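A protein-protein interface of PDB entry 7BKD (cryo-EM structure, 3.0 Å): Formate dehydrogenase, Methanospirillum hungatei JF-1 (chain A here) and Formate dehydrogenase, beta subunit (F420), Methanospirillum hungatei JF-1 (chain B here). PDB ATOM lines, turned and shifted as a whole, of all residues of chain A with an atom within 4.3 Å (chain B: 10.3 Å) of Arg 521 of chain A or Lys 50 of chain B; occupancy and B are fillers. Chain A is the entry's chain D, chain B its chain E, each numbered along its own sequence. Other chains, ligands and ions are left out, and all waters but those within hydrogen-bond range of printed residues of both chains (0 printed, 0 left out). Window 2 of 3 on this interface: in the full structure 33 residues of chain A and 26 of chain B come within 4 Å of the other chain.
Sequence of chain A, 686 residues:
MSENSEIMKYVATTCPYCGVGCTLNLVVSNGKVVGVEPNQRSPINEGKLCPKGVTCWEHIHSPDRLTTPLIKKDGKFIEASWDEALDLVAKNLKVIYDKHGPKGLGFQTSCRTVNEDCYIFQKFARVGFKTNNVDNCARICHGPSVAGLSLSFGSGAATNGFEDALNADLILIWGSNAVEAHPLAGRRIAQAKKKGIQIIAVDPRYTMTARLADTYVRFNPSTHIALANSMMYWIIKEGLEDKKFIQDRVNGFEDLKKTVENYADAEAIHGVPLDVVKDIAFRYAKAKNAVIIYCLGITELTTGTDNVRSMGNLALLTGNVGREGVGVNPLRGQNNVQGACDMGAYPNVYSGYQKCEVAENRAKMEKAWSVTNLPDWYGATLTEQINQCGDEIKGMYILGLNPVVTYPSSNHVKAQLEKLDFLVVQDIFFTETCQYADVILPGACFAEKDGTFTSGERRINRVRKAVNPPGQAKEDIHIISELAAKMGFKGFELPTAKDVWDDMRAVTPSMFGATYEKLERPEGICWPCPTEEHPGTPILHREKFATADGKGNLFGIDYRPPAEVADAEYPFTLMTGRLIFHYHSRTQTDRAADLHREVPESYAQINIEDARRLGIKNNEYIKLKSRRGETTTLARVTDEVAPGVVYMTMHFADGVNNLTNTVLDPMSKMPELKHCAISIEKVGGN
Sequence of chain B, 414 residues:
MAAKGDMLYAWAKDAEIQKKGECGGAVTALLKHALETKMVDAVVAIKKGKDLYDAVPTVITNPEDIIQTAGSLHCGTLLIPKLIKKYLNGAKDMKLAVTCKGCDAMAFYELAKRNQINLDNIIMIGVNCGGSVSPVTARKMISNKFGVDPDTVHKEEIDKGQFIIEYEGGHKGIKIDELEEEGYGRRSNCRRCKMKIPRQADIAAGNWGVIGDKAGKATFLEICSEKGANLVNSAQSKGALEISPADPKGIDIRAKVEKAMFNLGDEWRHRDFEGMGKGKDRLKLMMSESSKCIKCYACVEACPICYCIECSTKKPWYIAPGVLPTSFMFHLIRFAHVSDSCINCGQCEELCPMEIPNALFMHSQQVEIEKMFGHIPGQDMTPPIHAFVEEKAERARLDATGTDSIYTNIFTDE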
ATOM      1  N   ALA A  12       1.488 -31.999 -33.340  1.00  0.00           N
ATOM      2  CA  ALA A  12       1.268 -30.689 -33.931  1.00  0.00           C
ATOM      3  C   ALA A  12       2.561 -30.158 -34.535  1.00  0.00           C
ATOM      4  O   ALA A  12       3.584 -30.072 -33.853  1.00  0.00           O
ATOM      5  CB  ALA A  12       0.736 -29.717 -32.882  1.00  0.00           C
ATOM      6  N   ARG A 464       7.805 -30.168 -34.491  1.00  0.00           N
ATOM      7  CA  ARG A 464       7.952 -31.196 -33.475  1.00  0.00           C
ATOM      8  C   ARG A 464       8.367 -32.520 -34.099  1.00  0.00           C
ATOM      9  O   ARG A 464       8.023 -32.824 -35.243  1.00  0.00           O
ATOM     10  CB  ARG A 464       6.657 -31.378 -32.691  1.00  0.00           C
ATOM     11  CG  ARG A 464       6.226 -30.126 -31.969  1.00  0.00           C
ATOM     12  CD  ARG A 464       5.133 -30.404 -30.970  1.00  0.00           C
ATOM     13  NE  ARG A 464       4.944 -29.281 -30.060  1.00  0.00           N
ATOM     14  CZ  ARG A 464       4.393 -28.124 -30.403  1.00  0.00           C
ATOM     15  NH1 ARG A 464       3.966 -27.929 -31.641  1.00  0.00           N
ATOM     16  NH2 ARG A 464       4.262 -27.160 -29.506  1.00  0.00           N
ATOM     17  N   LYS A 518       7.668 -20.072 -24.081  1.00  0.00           N
ATOM     18  CA  LYS A 518       6.692 -19.204 -24.725  1.00  0.00           C
ATOM     19  C   LYS A 518       6.271 -19.727 -26.090  1.00  0.00           C
ATOM     20  O   LYS A 518       5.136 -19.492 -26.513  1.00  0.00           O
ATOM     21  CB  LYS A 518       7.248 -17.789 -24.865  1.00  0.00           C
ATOM     22  CG  LYS A 518       7.344 -17.031 -23.558  1.00  0.00           C
ATOM     23  CD  LYS A 518       7.959 -15.664 -23.766  1.00  0.00           C
ATOM     24  CE  LYS A 518       6.995 -14.736 -24.471  1.00  0.00           C
ATOM     25  NZ  LYS A 518       7.581 -13.390 -24.678  1.00  0.00           N
ATOM     26  N   LEU A 519       7.162 -20.425 -26.791  1.00  0.00           N
ATOM     27  CA  LEU A 519       6.839 -20.944 -28.112  1.00  0.00           C
ATOM     28  C   LEU A 519       5.981 -22.198 -28.063  1.00  0.00           C
ATOM     29  O   LEU A 519       5.449 -22.599 -29.101  1.00  0.00           O
ATOM     30  CB  LEU A 519       8.118 -21.235 -28.893  1.00  0.00           C
ATOM     31  CG  LEU A 519       8.954 -20.008 -29.249  1.00  0.00           C
ATOM     32  CD1 LEU A 519      10.175 -20.408 -30.050  1.00  0.00           C
ATOM     33  CD2 LEU A 519       8.117 -19.013 -30.011  1.00  0.00           C
ATOM     34  N   GLU A 520       5.838 -22.826 -26.900  1.00  0.00           N
ATOM     35  CA  GLU A 520       4.957 -23.977 -26.782  1.00  0.00           C
ATOM     36  C   GLU A 520       3.487 -23.590 -26.844  1.00  0.00           C
ATOM     37  O   GLU A 520       2.641 -24.456 -27.084  1.00  0.00           O
ATOM     38  CB  GLU A 520       5.246 -24.727 -25.480  1.00  0.00           C
ATOM     39  CG  GLU A 520       4.684 -26.142 -25.418  1.00  0.00           C
ATOM     40  CD  GLU A 520       5.358 -27.103 -26.385  1.00  0.00           C
ATOM     41  OE1 GLU A 520       6.335 -26.708 -27.055  1.00  0.00           O
ATOM     42  OE2 GLU A 520       4.906 -28.264 -26.476  1.00  0.00           O
ATOM     43  N   ARG A 521       3.167 -22.325 -26.635  1.00  0.00           N
ATOM     44  CA  ARG A 521       1.810 -21.840 -26.830  1.00  0.00           C
ATOM     45  C   ARG A 521       1.456 -21.876 -28.316  1.00  0.00           C
ATOM     46  O   ARG A 521       2.310 -21.605 -29.161  1.00  0.00           O
ATOM     47  CB  ARG A 521       1.669 -20.416 -26.299  1.00  0.00           C
ATOM     48  CG  ARG A 521       1.868 -20.265 -24.796  1.00  0.00           C
ATOM     49  CD  ARG A 521       0.784 -20.971 -23.995  1.00  0.00           C
ATOM     50  NE  ARG A 521       1.078 -22.381 -23.761  1.00  0.00           N
ATOM     51  CZ  ARG A 521       0.190 -23.262 -23.312  1.00  0.00           C
ATOM     52  NH1 ARG A 521      -1.050 -22.879 -23.049  1.00  0.00           N
ATOM     53  NH2 ARG A 521       0.543 -24.526 -23.127  1.00  0.00           N
ATOM     54  N   PRO A 522       0.212 -22.214 -28.657  1.00  0.00           N
ATOM     55  CA  PRO A 522      -0.162 -22.278 -30.078  1.00  0.00           C
ATOM     56  C   PRO A 522      -0.014 -20.960 -30.810  1.00  0.00           C
ATOM     57  O   PRO A 522       0.223 -20.961 -32.022  1.00  0.00           O
ATOM     58  CB  PRO A 522      -1.627 -22.731 -30.035  1.00  0.00           C
ATOM     59  CG  PRO A 522      -1.814 -23.340 -28.696  1.00  0.00           C
ATOM     60  CD  PRO A 522      -0.871 -22.656 -27.768  1.00  0.00           C
ATOM     61  N   GLU A 523      -0.185 -19.848 -30.122  1.00  0.00           N
ATOM     62  CA  GLU A 523      -0.162 -18.546 -30.812  1.00  0.00           C
ATOM     63  C   GLU A 523       1.234 -18.264 -31.346  1.00  0.00           C
ATOM     64  O   GLU A 523       1.328 -17.475 -32.275  1.00  0.00           O
ATOM     65  CB  GLU A 523      -0.595 -17.457 -29.844  1.00  0.00           C
ATOM     66  CG  GLU A 523      -2.099 -17.342 -29.691  1.00  0.00           C
ATOM     67  CD  GLU A 523      -2.721 -18.344 -28.736  1.00  0.00           C
ATOM     68  OE1 GLU A 523      -2.055 -18.711 -27.747  1.00  0.00           O
ATOM     69  OE2 GLU A 523      -3.865 -18.760 -28.989  1.00  0.00           O
ATOM     70  N   GLY A 524       2.281 -18.848 -30.758  1.00  0.00           N
ATOM     71  CA  GLY A 524       3.669 -18.560 -31.177  1.00  0.00           C
ATOM     72  C   GLY A 524       4.113 -17.191 -30.711  1.00  0.00           C
ATOM     73  O   GLY A 524       3.467 -16.651 -29.812  1.00  0.00           O
ATOM     74  N   LYS B  47      -8.932 -35.721 -25.057  1.00  0.00           N
ATOM     75  CA  LYS B  47      -8.184 -35.176 -23.937  1.00  0.00           C
ATOM     76  C   LYS B  47      -7.686 -33.781 -24.279  1.00  0.00           C
ATOM     77  O   LYS B  47      -7.621 -33.385 -25.444  1.00  0.00           O
ATOM     78  CB  LYS B  47      -7.011 -36.081 -23.544  1.00  0.00           C
ATOM     79  CG  LYS B  47      -5.978 -36.276 -24.622  1.00  0.00           C
ATOM     80  CD  LYS B  47      -4.640 -36.661 -24.025  1.00  0.00           C
ATOM     81  CE  LYS B  47      -3.565 -36.745 -25.094  1.00  0.00           C
ATOM     82  NZ  LYS B  47      -3.327 -35.434 -25.756  1.00  0.00           N
ATOM     83  N   LYS B  48      -7.358 -33.023 -23.239  1.00  0.00           N
ATOM     84  CA  LYS B  48      -6.843 -31.679 -23.436  1.00  0.00           C
ATOM     85  C   LYS B  48      -5.473 -31.725 -24.096  1.00  0.00           C
ATOM     86  O   LYS B  48      -4.653 -32.599 -23.804  1.00  0.00           O
ATOM     87  CB  LYS B  48      -6.746 -30.942 -22.104  1.00  0.00           C
ATOM     88  CG  LYS B  48      -8.075 -30.625 -21.458  1.00  0.00           C
ATOM     89  CD  LYS B  48      -7.871 -29.870 -20.160  1.00  0.00           C
ATOM     90  CE  LYS B  48      -9.192 -29.563 -19.487  1.00  0.00           C
ATOM     91  NZ  LYS B  48      -8.995 -28.833 -18.205  1.00  0.00           N
ATOM     92  N   GLY B  49      -5.225 -30.775 -24.985  1.00  0.00           N
ATOM     93  CA  GLY B  49      -3.917 -30.639 -25.585  1.00  0.00           C
ATOM     94  C   GLY B  49      -3.063 -29.646 -24.827  1.00  0.00           C
ATOM     95  O   GLY B  49      -2.687 -29.888 -23.678  1.00  0.00           O
ATOM     96  N   LYS B  50      -2.752 -28.520 -25.464  1.00  0.00           N
ATOM     97  CA  LYS B  50      -1.950 -27.497 -24.809  1.00  0.00           C
ATOM     98  C   LYS B  50      -2.761 -26.688 -23.803  1.00  0.00           C
ATOM     99  O   LYS B  50      -2.203 -26.202 -22.812  1.00  0.00           O
ATOM    100  CB  LYS B  50      -1.326 -26.583 -25.860  1.00  0.00           C
ATOM    101  CG  LYS B  50      -0.408 -27.322 -26.819  1.00  0.00           C
ATOM    102  CD  LYS B  50       0.020 -26.440 -27.975  1.00  0.00           C
ATOM    103  CE  LYS B  50       0.567 -27.266 -29.125  1.00  0.00           C
ATOM    104  NZ  LYS B  50       0.567 -26.503 -30.406  1.00  0.00           N
ATOM    105  N   ASP B  51      -4.060 -26.532 -24.032  1.00  0.00           N
ATOM    106  CA  ASP B  51      -4.932 -25.794 -23.127  1.00  0.00           C
ATOM    107  C   ASP B  51      -6.319 -26.426 -23.177  1.00  0.00           C
ATOM    108  O   ASP B  51      -6.503 -27.511 -23.735  1.00  0.00           O
ATOM    109  CB  ASP B  51      -4.919 -24.301 -23.479  1.00  0.00           C
ATOM    110  CG  ASP B  51      -5.451 -24.018 -24.869  1.00  0.00           C
ATOM    111  OD1 ASP B  51      -5.797 -24.973 -25.590  1.00  0.00           O
ATOM    112  OD2 ASP B  51      -5.508 -22.832 -25.252  1.00  0.00           O
ATOM    113  N   LEU B  52      -7.302 -25.755 -22.583  1.00  0.00           N
ATOM    114  CA  LEU B  52      -8.651 -26.303 -22.576  1.00  0.00           C
ATOM    115  C   LEU B  52      -9.399 -26.051 -23.876  1.00  0.00           C
ATOM    116  O   LEU B  52     -10.460 -26.648 -24.084  1.00  0.00           O
ATOM    117  CB  LEU B  52      -9.464 -25.741 -21.407  1.00  0.00           C
ATOM    118  CG  LEU B  52      -9.953 -24.294 -21.440  1.00  0.00           C
ATOM    119  CD1 LEU B  52     -11.020 -24.104 -20.387  1.00  0.00           C
ATOM    120  CD2 LEU B  52      -8.819 -23.318 -21.206  1.00  0.00           C
ATOM    121  N   TYR B  53      -8.886 -25.188 -24.747  1.00  0.00           N
ATOM    122  CA  TYR B  53      -9.466 -25.012 -26.068  1.00  0.00           C
ATOM    123  C   TYR B  53      -8.913 -25.994 -27.089  1.00  0.00           C
ATOM    124  O   TYR B  53      -9.384 -26.008 -28.229  1.00  0.00           O
ATOM    125  CB  TYR B  53      -9.229 -23.588 -26.569  1.00  0.00           C
ATOM    126  CG  TYR B  53      -9.500 -22.516 -25.549  1.00  0.00           C
ATOM    127  CD1 TYR B  53      -8.515 -21.614 -25.191  1.00  0.00           C
ATOM    128  CD2 TYR B  53     -10.743 -22.395 -24.954  1.00  0.00           C
ATOM    129  CE1 TYR B  53      -8.756 -20.630 -24.267  1.00  0.00           C
ATOM    130  CE2 TYR B  53     -10.993 -21.411 -24.027  1.00  0.00           C
ATOM    131  CZ  TYR B  53      -9.995 -20.532 -23.688  1.00  0.00           C
ATOM    132  OH  TYR B  53     -10.232 -19.548 -22.763  1.00  0.00           O
ATOM    133  N   ASP B  54      -7.933 -26.805 -26.714  1.00  0.00           N
ATOM    134  CA  ASP B  54      -7.311 -27.763 -27.618  1.00  0.00           C
ATOM    135  C   ASP B  54      -7.788 -29.153 -27.223  1.00  0.00           C
ATOM    136  O   ASP B  54      -7.358 -29.695 -26.201  1.00  0.00           O
ATOM    137  CB  ASP B  54      -5.790 -27.657 -27.552  1.00  0.00           C
ATOM    138  CG  ASP B  54      -5.094 -28.496 -28.608  1.00  0.00           C
ATOM    139  OD1 ASP B  54      -3.861 -28.363 -28.749  1.00  0.00           O
ATOM    140  OD2 ASP B  54      -5.773 -29.276 -29.308  1.00  0.00           O
ATOM    141  N   ALA B  55      -8.672 -29.723 -28.030  1.00  0.00           N
ATOM    142  CA  ALA B  55      -9.196 -31.062 -27.812  1.00  0.00           C
ATOM    143  C   ALA B  55      -8.549 -32.004 -28.811  1.00  0.00           C
ATOM    144  O   ALA B  55      -8.579 -31.744 -30.018  1.00  0.00           O
ATOM    145  CB  ALA B  55     -10.716 -31.088 -27.964  1.00  0.00           C
ATOM    146  N   VAL B  56      -7.968 -33.091 -28.317  1.00  0.00           N
ATOM    147  CA  VAL B  56      -7.190 -34.015 -29.127  1.00  0.00           C
ATOM    148  C   VAL B  56      -7.779 -35.406 -28.955  1.00  0.00           C
ATOM    149  O   VAL B  56      -7.920 -35.869 -27.821  1.00  0.00           O
ATOM    150  CB  VAL B  56      -5.699 -34.016 -28.747  1.00  0.00           C
ATOM    151  CG1 VAL B  56      -4.955 -35.055 -29.549  1.00  0.00           C
ATOM    152  CG2 VAL B  56      -5.105 -32.647 -28.976  1.00  0.00           C
ATOM    153  N   LEU B  73     -15.025 -31.066 -23.086  1.00  0.00           N
ATOM    154  CA  LEU B  73     -14.419 -29.897 -23.712  1.00  0.00           C
ATOM    155  C   LEU B  73     -15.408 -29.349 -24.725  1.00  0.00           C
ATOM    156  O   LEU B  73     -15.595 -29.937 -25.793  1.00  0.00           O
ATOM    157  CB  LEU B  73     -13.095 -30.249 -24.382  1.00  0.00           C
ATOM    158  CG  LEU B  73     -12.080 -30.951 -23.487  1.00  0.00           C
ATOM    159  CD1 LEU B  73     -10.902 -31.414 -24.304  1.00  0.00           C
ATOM    160  CD2 LEU B  73     -11.636 -30.023 -22.380  1.00  0.00           C
ATOM    161  N   ARG B 139     -12.114 -18.117 -27.926  1.00  0.00           N
ATOM    162  CA  ARG B 139     -11.146 -17.147 -27.430  1.00  0.00           C
ATOM    163  C   ARG B 139     -11.535 -15.732 -27.825  1.00  0.00           C
ATOM    164  O   ARG B 139     -11.333 -14.791 -27.053  1.00  0.00           O
ATOM    165  CB  ARG B 139      -9.750 -17.486 -27.936  1.00  0.00           C
ATOM    166  CG  ARG B 139      -9.204 -18.777 -27.377  1.00  0.00           C
ATOM    167  CD  ARG B 139      -7.843 -19.077 -27.954  1.00  0.00           C
ATOM    168  NE  ARG B 139      -6.866 -18.068 -27.554  1.00  0.00           N
ATOM    169  CZ  ARG B 139      -6.153 -18.119 -26.437  1.00  0.00           C
ATOM    170  NH1 ARG B 139      -6.309 -19.126 -25.595  1.00  0.00           N
ATOM    171  NH2 ARG B 139      -5.288 -17.158 -26.159  1.00  0.00           N
ATOM    172  N   ASP B 149      -8.741 -12.107 -20.355  1.00  0.00           N
ATOM    173  CA  ASP B 149      -7.699 -12.774 -21.121  1.00  0.00           C
ATOM    174  C   ASP B 149      -8.005 -14.265 -21.193  1.00  0.00           C
ATOM    175  O   ASP B 149      -8.200 -14.901 -20.153  1.00  0.00           O
ATOM    176  CB  ASP B 149      -6.333 -12.542 -20.488  1.00  0.00           C
ATOM    177  CG  ASP B 149      -5.216 -12.529 -21.510  1.00  0.00           C
ATOM    178  OD1 ASP B 149      -5.460 -12.096 -22.654  1.00  0.00           O
ATOM    179  OD2 ASP B 149      -4.092 -12.955 -21.169  1.00  0.00           O
ATOM    180  N   PRO B 150      -8.068 -14.851 -22.389  1.00  0.00           N
ATOM    181  CA  PRO B 150      -8.454 -16.267 -22.490  1.00  0.00           C
ATOM    182  C   PRO B 150      -7.515 -17.213 -21.769  1.00  0.00           C
ATOM    183  O   PRO B 150      -7.956 -18.268 -21.298  1.00  0.00           O
ATOM    184  CB  PRO B 150      -8.456 -16.521 -24.003  1.00  0.00           C
ATOM    185  CG  PRO B 150      -8.558 -15.177 -24.623  1.00  0.00           C
ATOM    186  CD  PRO B 150      -7.848 -14.244 -23.709  1.00  0.00           C
ATOM    187  N   ASP B 151      -6.228 -16.876 -21.674  1.00  0.00           N
ATOM    188  CA  ASP B 151      -5.273 -17.778 -21.042  1.00  0.00           C
ATOM    189  C   ASP B 151      -5.584 -17.988 -19.570  1.00  0.00           C
ATOM    190  O   ASP B 151      -5.270 -19.045 -19.014  1.00  0.00           O
ATOM    191  CB  ASP B 151      -3.857 -17.235 -21.211  1.00  0.00           C
ATOM    192  CG  ASP B 151      -3.443 -17.144 -22.661  1.00  0.00           C
ATOM    193  OD1 ASP B 151      -2.988 -18.167 -23.217  1.00  0.00           O
ATOM    194  OD2 ASP B 151      -3.577 -16.051 -23.251  1.00  0.00           O
ATOM    195  N   THR B 152      -6.200 -17.000 -18.924  1.00  0.00           N
ATOM    196  CA  THR B 152      -6.493 -17.090 -17.501  1.00  0.00           C
ATOM    197  C   THR B 152      -7.705 -17.957 -17.195  1.00  0.00           C
ATOM    198  O   THR B 152      -7.967 -18.225 -16.019  1.00  0.00           O
ATOM    199  CB  THR B 152      -6.712 -15.693 -16.932  1.00  0.00           C
ATOM    200  OG1 THR B 152      -8.026 -15.244 -17.273  1.00  0.00           O
ATOM    201  CG2 THR B 152      -5.695 -14.729 -17.508  1.00  0.00           C
ATOM    202  N   VAL B 153      -8.447 -18.397 -18.211  1.00  0.00           N
ATOM    203  CA  VAL B 153      -9.672 -19.148 -17.975  1.00  0.00           C
ATOM    204  C   VAL B 153      -9.330 -20.554 -17.506  1.00  0.00           C
ATOM    205  O   VAL B 153      -8.523 -21.255 -18.126  1.00  0.00           O
ATOM    206  CB  VAL B 153     -10.537 -19.179 -19.242  1.00  0.00           C
ATOM    207  CG1 VAL B 153     -11.801 -19.971 -18.994  1.00  0.00           C
ATOM    208  CG2 VAL B 153     -10.875 -17.771 -19.685  1.00  0.00           C
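The guanidinium group (NH2) of Arg 521 of chain A lies within hydrogen-bond range of the backbone carbonyl oxygen (O) of Lys 50 of chain B (3.2 Å).
The guanidinium group of Arg 139 of chain B is in salt-bridge range of the side-chain carboxylate of Glu 523 of chain A (3.4 Å).
The backbone NH (N) of Lys 50 of chain B sits at hydrogen-bond distance from the side-chain carboxylate (OD1) of Asp 54 of chain B.
OD2 of Asp 51 of chain B is in salt-bridge range of NH1 of Arg 139 of chain B (3.8 Å).
NH2 of Arg 139 of chain B lies within salt-bridge range of OD2 of Asp 151 of chain B (3.6 Å).
O of Ala 12 of chain A lies within hydrogen-bond range of NH1 of Arg 464 of chain A, 3.1 Å away.
The guanidinium group (NH2) of Arg 464 of chain A lies within salt-bridge range of the side-chain carboxylate (OE1) of Glu 520 of chain A (3.2 Å).
NH2 of Arg 464 of chain A touches CE of Lys 50 of chain B, at 3.7 Å.
O of Glu 520 of chain A touches CD of Lys 50 of chain B, at 3.4 Å.
Pro 522 of chain A touches Lys 50 of chain B.
Of the printed residues of chain B, Arg 464 of chain A touches Lys 50.
Of chain B, only Lys 50 (3.4 Å) comes within 4 Å of Glu 520 of chain A.
Arg 521 of chain A touches one residue of chain B.
Of chain B, only Lys 50 comes within 4 Å of Pro 522 of chain A.
Glu 523 of chain A touches just one residue of chain B: Arg 139 (3.4 Å).
No residue of chain B comes within 4 Å of Gly 524 of chain A.
Of chain A, only Arg 464 (3.7 Å), Glu 520 (3.4 Å), Arg 521 (3.2 Å) and Pro 522 (3.7 Å) come within 4 Å of Lys 50 of chain B.
Tyr 53 of chain B touches none of the printed residues of chain A.
Printed residues of chain A within 4 Å of Arg 139 of chain B: Glu 523.
Printed residues of chain A that touch a printed residue of chain B: Arg 464, Glu 520, Arg 521, Pro 522 and Glu 523.
Of the 17 printed residues of chain B, 2 touch a printed residue of chain A.
Along chain B the printed residues that touch a printed residue of chain A span positions 50 to 139.
Among the printed residues, Asp or Glu carboxylates within 4 Å of a Lys or Arg side-chain nitrogen of the other chain: Glu 523 of chain A with Arg 139 of chain B.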
